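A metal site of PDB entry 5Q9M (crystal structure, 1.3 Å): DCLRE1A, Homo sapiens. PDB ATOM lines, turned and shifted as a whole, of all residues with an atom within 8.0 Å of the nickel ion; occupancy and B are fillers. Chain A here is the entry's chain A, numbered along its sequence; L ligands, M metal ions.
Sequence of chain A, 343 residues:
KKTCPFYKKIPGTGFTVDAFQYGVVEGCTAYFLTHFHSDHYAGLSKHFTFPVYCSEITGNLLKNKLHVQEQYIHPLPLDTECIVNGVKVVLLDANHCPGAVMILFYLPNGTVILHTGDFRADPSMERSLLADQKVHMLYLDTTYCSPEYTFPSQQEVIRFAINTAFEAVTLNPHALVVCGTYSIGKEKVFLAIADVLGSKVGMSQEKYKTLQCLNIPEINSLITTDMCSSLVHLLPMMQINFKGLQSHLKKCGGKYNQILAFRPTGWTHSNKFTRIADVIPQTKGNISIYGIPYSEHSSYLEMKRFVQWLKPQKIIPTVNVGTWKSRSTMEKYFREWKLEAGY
The nickel ion is bound by an oxygen (O3) of the ligand (2.1 Å), an oxygen (O2) of the ligand (2.2 Å), the side-chain carboxylate (OD2) of Asp 118 (2.2 Å), a ring nitrogen (NE2) of His 35 (2.3 Å), a ring nitrogen (ND1) of His 37 (2.3 Å) and a ring nitrogen (NE2) of His 96 (2.3 Å).
The nickel ion has six donor atoms within binding distance.
NE2 of His 40 lies close to OD2 of Asp 118.
ND1 of His 35 sits at hydrogen-bond distance from OG1 of Thr 34 (2.9 Å).
The backbone carbonyl oxygen of Ile 184 sits at hydrogen-bond distance from a ring nitrogen (NE2) of His 37, 2.9 Å away.
O of Glu 296 is in hydrogen-bond range of ND1 of His 96 (2.8 Å).
Within 4 Å of the nickel ion: His 35, His 37, His 96 and Asp 118.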
ATOM      1  N   ASP A  18     -27.895  28.531 -11.318  1.00  0.00           N
ATOM      2  CA  ASP A  18     -26.712  28.100 -12.121  1.00  0.00           C
ATOM      3  C   ASP A  18     -27.123  27.244 -13.392  1.00  0.00           C
ATOM      4  O   ASP A  18     -26.528  26.172 -13.689  1.00  0.00           O
ATOM      5  CB  ASP A  18     -25.698  27.421 -11.240  1.00  0.00           C
ATOM      6  CG  ASP A  18     -25.201  28.308 -10.083  1.00  0.00           C
ATOM      7  OD1 ASP A  18     -25.427  29.538 -10.127  1.00  0.00           O
ATOM      8  OD2 ASP A  18     -24.523  27.711  -9.207  1.00  0.00           O
ATOM      9  N   THR A  34     -24.827  31.763  -8.476  1.00  0.00           N
ATOM     10  CA  THR A  34     -24.177  31.712  -7.157  1.00  0.00           C
ATOM     11  C   THR A  34     -22.774  32.328  -7.142  1.00  0.00           C
ATOM     12  O   THR A  34     -22.385  32.935  -6.140  1.00  0.00           O
ATOM     13  CB  THR A  34     -24.150  30.301  -6.560  1.00  0.00           C
ATOM     14  OG1 THR A  34     -23.340  29.395  -7.364  1.00  0.00           O
ATOM     15  CG2 THR A  34     -25.535  29.715  -6.319  1.00  0.00           C
ATOM     16  N   HIS A  35     -22.026  32.147  -8.265  1.00  0.00           N
ATOM     17  CA  HIS A  35     -20.626  32.580  -8.323  1.00  0.00           C
ATOM     18  C   HIS A  35     -20.108  32.536  -9.733  1.00  0.00           C
ATOM     19  O   HIS A  35     -20.633  31.754 -10.567  1.00  0.00           O
ATOM     20  CB  HIS A  35     -19.732  31.803  -7.298  1.00  0.00           C
ATOM     21  CG  HIS A  35     -19.480  30.368  -7.597  1.00  0.00           C
ATOM     22  ND1 HIS A  35     -20.443  29.374  -7.531  1.00  0.00           N
ATOM     23  CD2 HIS A  35     -18.330  29.726  -7.966  1.00  0.00           C
ATOM     24  CE1 HIS A  35     -19.840  28.209  -7.791  1.00  0.00           C
ATOM     25  NE2 HIS A  35     -18.572  28.414  -8.015  1.00  0.00           N
ATOM     26  N   PHE A  36     -19.028  33.291  -9.963  1.00  0.00           N
ATOM     27  CA  PHE A  36     -18.402  33.373 -11.321  1.00  0.00           C
ATOM     28  C   PHE A  36     -17.347  32.283 -11.568  1.00  0.00           C
ATOM     29  O   PHE A  36     -16.112  32.611 -11.681  1.00  0.00           O
ATOM     30  CB  PHE A  36     -17.802  34.799 -11.514  1.00  0.00           C
ATOM     31  CG  PHE A  36     -17.517  35.151 -12.963  1.00  0.00           C
ATOM     32  CD1 PHE A  36     -18.548  35.467 -13.835  1.00  0.00           C
ATOM     33  CD2 PHE A  36     -16.202  35.212 -13.402  1.00  0.00           C
ATOM     34  CE1 PHE A  36     -18.249  35.780 -15.199  1.00  0.00           C
ATOM     35  CE2 PHE A  36     -15.888  35.566 -14.732  1.00  0.00           C
ATOM     36  CZ  PHE A  36     -16.884  35.853 -15.608  1.00  0.00           C
ATOM     37  N   HIS A  37     -17.753  31.029 -11.672  1.00  0.00           N
ATOM     38  CA  HIS A  37     -16.942  29.889 -12.133  1.00  0.00           C
ATOM     39  C   HIS A  37     -17.656  29.302 -13.373  1.00  0.00           C
ATOM     40  O   HIS A  37     -18.888  29.149 -13.398  1.00  0.00           O
ATOM     41  CB  HIS A  37     -16.746  28.795 -11.068  1.00  0.00           C
ATOM     42  CG  HIS A  37     -15.651  29.099 -10.049  1.00  0.00           C
ATOM     43  ND1 HIS A  37     -15.518  28.418  -8.849  1.00  0.00           N
ATOM     44  CD2 HIS A  37     -14.602  29.963 -10.088  1.00  0.00           C
ATOM     45  CE1 HIS A  37     -14.467  28.863  -8.186  1.00  0.00           C
ATOM     46  NE2 HIS A  37     -13.906  29.812  -8.916  1.00  0.00           N
ATOM     47  N   SER A  38     -16.831  28.922 -14.365  1.00  0.00           N
ATOM     48  CA  SER A  38     -17.342  28.607 -15.716  1.00  0.00           C
ATOM     49  C   SER A  38     -18.312  27.460 -15.717  1.00  0.00           C
ATOM     50  O   SER A  38     -19.280  27.585 -16.534  1.00  0.00           O
ATOM     51  CB  SER A  38     -16.177  28.492 -16.725  1.00  0.00           C
ATOM     52  OG  SER A  38     -15.328  27.409 -16.386  1.00  0.00           O
ATOM     53  N   ASP A  39     -18.163  26.424 -14.906  1.00  0.00           N
ATOM     54  CA  ASP A  39     -19.167  25.294 -14.920  1.00  0.00           C
ATOM     55  C   ASP A  39     -20.549  25.815 -14.516  1.00  0.00           C
ATOM     56  O   ASP A  39     -21.579  25.194 -14.850  1.00  0.00           O
ATOM     57  CB  ASP A  39     -18.777  24.167 -14.018  1.00  0.00           C
ATOM     58  CG  ASP A  39     -17.705  23.158 -14.640  1.00  0.00           C
ATOM     59  OD1 ASP A  39     -17.270  23.365 -15.787  1.00  0.00           O
ATOM     60  OD2 ASP A  39     -17.332  22.254 -13.872  1.00  0.00           O
ATOM     61  N   HIS A  40     -20.616  26.910 -13.727  1.00  0.00           N
ATOM     62  CA  HIS A  40     -21.884  27.488 -13.237  1.00  0.00           C
ATOM     63  C   HIS A  40     -22.430  28.580 -14.097  1.00  0.00           C
ATOM     64  O   HIS A  40     -23.688  28.647 -14.265  1.00  0.00           O
ATOM     65  CB  HIS A  40     -21.641  28.004 -11.763  1.00  0.00           C
ATOM     66  CG  HIS A  40     -21.251  26.920 -10.853  1.00  0.00           C
ATOM     67  ND1 HIS A  40     -22.120  26.327  -9.958  1.00  0.00           N
ATOM     68  CD2 HIS A  40     -20.080  26.250 -10.701  1.00  0.00           C
ATOM     69  CE1 HIS A  40     -21.526  25.342  -9.334  1.00  0.00           C
ATOM     70  NE2 HIS A  40     -20.268  25.291  -9.749  1.00  0.00           N
ATOM     71  N   HIS A  96     -16.320  30.677  -0.450  1.00  0.00           N
ATOM     72  CA  HIS A  96     -15.800  29.980  -1.663  1.00  0.00           C
ATOM     73  C   HIS A  96     -14.856  30.980  -2.283  1.00  0.00           C
ATOM     74  O   HIS A  96     -13.805  31.282  -1.610  1.00  0.00           O
ATOM     75  CB  HIS A  96     -16.969  29.459  -2.519  1.00  0.00           C
ATOM     76  CG  HIS A  96     -16.593  28.643  -3.755  1.00  0.00           C
ATOM     77  ND1 HIS A  96     -15.743  27.551  -3.684  1.00  0.00           N
ATOM     78  CD2 HIS A  96     -16.896  28.771  -5.065  1.00  0.00           C
ATOM     79  CE1 HIS A  96     -15.591  27.039  -4.922  1.00  0.00           C
ATOM     80  NE2 HIS A  96     -16.325  27.723  -5.773  1.00  0.00           N
ATOM     81  N   CYS A  97     -15.066  31.439  -3.508  1.00  0.00           N
ATOM     82  CA  CYS A  97     -14.282  32.520  -4.162  1.00  0.00           C
ATOM     83  C   CYS A  97     -14.936  33.871  -3.977  1.00  0.00           C
ATOM     84  O   CYS A  97     -16.077  33.956  -3.472  1.00  0.00           O
ATOM     85  CB  CYS A  97     -14.175  32.149  -5.660  1.00  0.00           C
ATOM     86  SG  CYS A  97     -15.794  32.142  -6.568  1.00  0.00           S
ATOM     87  N   ALA A 100     -18.996  34.749  -4.155  1.00  0.00           N
ATOM     88  CA  ALA A 100     -19.765  33.513  -4.068  1.00  0.00           C
ATOM     89  C   ALA A 100     -20.776  33.578  -2.901  1.00  0.00           C
ATOM     90  O   ALA A 100     -20.430  33.969  -1.772  1.00  0.00           O
ATOM     91  CB  ALA A 100     -18.872  32.326  -3.922  1.00  0.00           C
ATOM     92  N   GLY A 117     -24.830  26.751  -3.220  1.00  0.00           N
ATOM     93  CA  GLY A 117     -23.884  26.951  -4.287  1.00  0.00           C
ATOM     94  C   GLY A 117     -22.676  26.085  -4.066  1.00  0.00           C
ATOM     95  O   GLY A 117     -22.791  24.979  -3.552  1.00  0.00           O
ATOM     96  N   ASP A 118     -21.508  26.582  -4.447  1.00  0.00           N
ATOM     97  CA  ASP A 118     -20.233  26.009  -3.960  1.00  0.00           C
ATOM     98  C   ASP A 118     -19.807  26.692  -2.636  1.00  0.00           C
ATOM     99  O   ASP A 118     -19.931  27.927  -2.549  1.00  0.00           O
ATOM    100  CB  ASP A 118     -19.098  26.163  -4.979  1.00  0.00           C
ATOM    101  CG  ASP A 118     -19.128  25.212  -6.175  1.00  0.00           C
ATOM    102  OD1 ASP A 118     -19.899  24.244  -6.179  1.00  0.00           O
ATOM    103  OD2 ASP A 118     -18.294  25.376  -7.055  1.00  0.00           O
ATOM    104  N   PHE A 119     -19.428  25.924  -1.611  1.00  0.00           N
ATOM    105  CA  PHE A 119     -19.073  26.513  -0.323  1.00  0.00           C
ATOM    106  C   PHE A 119     -17.994  25.733   0.422  1.00  0.00           C
ATOM    107  O   PHE A 119     -17.780  24.552   0.183  1.00  0.00           O
ATOM    108  CB  PHE A 119     -20.366  26.741   0.584  1.00  0.00           C
ATOM    109  CG  PHE A 119     -20.867  25.587   1.463  1.00  0.00           C
ATOM    110  CD1 PHE A 119     -21.348  25.804   2.774  1.00  0.00           C
ATOM    111  CD2 PHE A 119     -20.929  24.283   0.972  1.00  0.00           C
ATOM    112  CE1 PHE A 119     -21.881  24.779   3.520  1.00  0.00           C
ATOM    113  CE2 PHE A 119     -21.425  23.232   1.760  1.00  0.00           C
ATOM    114  CZ  PHE A 119     -21.922  23.489   3.045  1.00  0.00           C
ATOM    115  N   ASP A 141     -23.518  21.363  -1.782  1.00  0.00           N
ATOM    116  CA  ASP A 141     -22.196  21.151  -2.508  1.00  0.00           C
ATOM    117  C   ASP A 141     -21.503  19.980  -1.796  1.00  0.00           C
ATOM    118  O   ASP A 141     -20.910  20.070  -0.725  1.00  0.00           O
ATOM    119  CB  ASP A 141     -21.324  22.395  -2.419  1.00  0.00           C
ATOM    120  CG  ASP A 141     -19.879  22.156  -2.813  1.00  0.00           C
ATOM    121  OD1 ASP A 141     -19.583  21.113  -3.413  1.00  0.00           O
ATOM    122  OD2 ASP A 141     -19.039  23.052  -2.522  1.00  0.00           O
ATOM    123  N   THR A 143     -18.955  18.126  -3.191  1.00  0.00           N
ATOM    124  CA  THR A 143     -17.691  17.855  -3.869  1.00  0.00           C
ATOM    125  C   THR A 143     -16.837  16.849  -3.151  1.00  0.00           C
ATOM    126  O   THR A 143     -16.385  15.830  -3.810  1.00  0.00           O
ATOM    127  CB  THR A 143     -16.919  19.196  -4.085  1.00  0.00           C
ATOM    128  OG1 THR A 143     -17.651  20.087  -4.927  1.00  0.00           O
ATOM    129  CG2 THR A 143     -15.573  18.926  -4.748  1.00  0.00           C
ATOM    130  N   SER A 183      -8.900  30.547 -12.742  1.00  0.00           N
ATOM    131  CA  SER A 183     -10.210  31.046 -12.405  1.00  0.00           C
ATOM    132  C   SER A 183     -10.041  32.030 -11.226  1.00  0.00           C
ATOM    133  O   SER A 183      -8.958  32.066 -10.593  1.00  0.00           O
ATOM    134  CB  SER A 183     -11.144  29.921 -11.894  1.00  0.00           C
ATOM    135  OG  SER A 183     -10.592  29.285 -10.769  1.00  0.00           O
ATOM    136  N   ILE A 184     -11.074  32.744 -10.865  1.00  0.00           N
ATOM    137  CA  ILE A 184     -11.055  33.475  -9.609  1.00  0.00           C
ATOM    138  C   ILE A 184     -11.088  32.496  -8.412  1.00  0.00           C
ATOM    139  O   ILE A 184     -11.468  31.299  -8.564  1.00  0.00           O
ATOM    140  CB  ILE A 184     -12.205  34.507  -9.435  1.00  0.00           C
ATOM    141  CG1 ILE A 184     -13.602  33.890  -9.329  1.00  0.00           C
ATOM    142  CG2 ILE A 184     -12.082  35.627 -10.471  1.00  0.00           C
ATOM    143  CD1 ILE A 184     -14.682  34.859  -8.873  1.00  0.00           C
ATOM    144  N   GLU A 296     -11.135  25.589  -1.493  1.00  0.00           N
ATOM    145  CA  GLU A 296     -12.345  26.452  -1.307  1.00  0.00           C
ATOM    146  C   GLU A 296     -13.682  25.653  -1.271  1.00  0.00           C
ATOM    147  O   GLU A 296     -14.769  26.226  -1.441  1.00  0.00           O
ATOM    148  CB  GLU A 296     -12.361  27.645  -2.239  1.00  0.00           C
ATOM    149  CG  GLU A 296     -11.209  28.701  -1.970  1.00  0.00           C
ATOM    150  CD  GLU A 296     -11.199  29.967  -2.830  1.00  0.00           C
ATOM    151  OE1 GLU A 296     -11.839  29.965  -3.912  1.00  0.00           O
ATOM    152  OE2 GLU A 296     -10.561  30.961  -2.358  1.00  0.00           O
ATOM    153  N   HIS A 297     -13.531  24.345  -1.024  1.00  0.00           N
ATOM    154  CA  HIS A 297     -14.694  23.483  -0.739  1.00  0.00           C
ATOM    155  C   HIS A 297     -14.580  22.831   0.632  1.00  0.00           C
ATOM    156  O   HIS A 297     -13.464  22.570   1.173  1.00  0.00           O
ATOM    157  CB  HIS A 297     -14.891  22.340  -1.792  1.00  0.00           C
ATOM    158  CG  HIS A 297     -15.194  22.804  -3.166  1.00  0.00           C
ATOM    159  ND1 HIS A 297     -16.470  23.038  -3.635  1.00  0.00           N
ATOM    160  CD2 HIS A 297     -14.379  22.955  -4.277  1.00  0.00           C
ATOM    161  CE1 HIS A 297     -16.420  23.388  -4.923  1.00  0.00           C
ATOM    162  NE2 HIS A 297     -15.173  23.367  -5.299  1.00  0.00           N
HETATM  163  C1  LIG L   1     -14.907  25.004  -9.758  1.00  0.00           C
HETATM  164  C2  LIG L   1     -14.671  24.729  -8.270  1.00  0.00           C
HETATM  165  C3  LIG L   1     -16.399  25.089 -10.148  1.00  0.00           C
HETATM  166  O1  LIG L   1     -13.973  23.812  -7.806  1.00  0.00           O
HETATM  167  O2  LIG L   1     -15.261  25.451  -7.494  1.00  0.00           O
HETATM  168  O3  LIG L   1     -17.185  25.877  -9.612  1.00  0.00           O
HETATM  169  O4  LIG L   1     -16.789  24.479 -11.196  1.00  0.00           O
HETATM  170 NI    NI M   1     -16.884  26.915  -7.831  1.00  0.00          NI
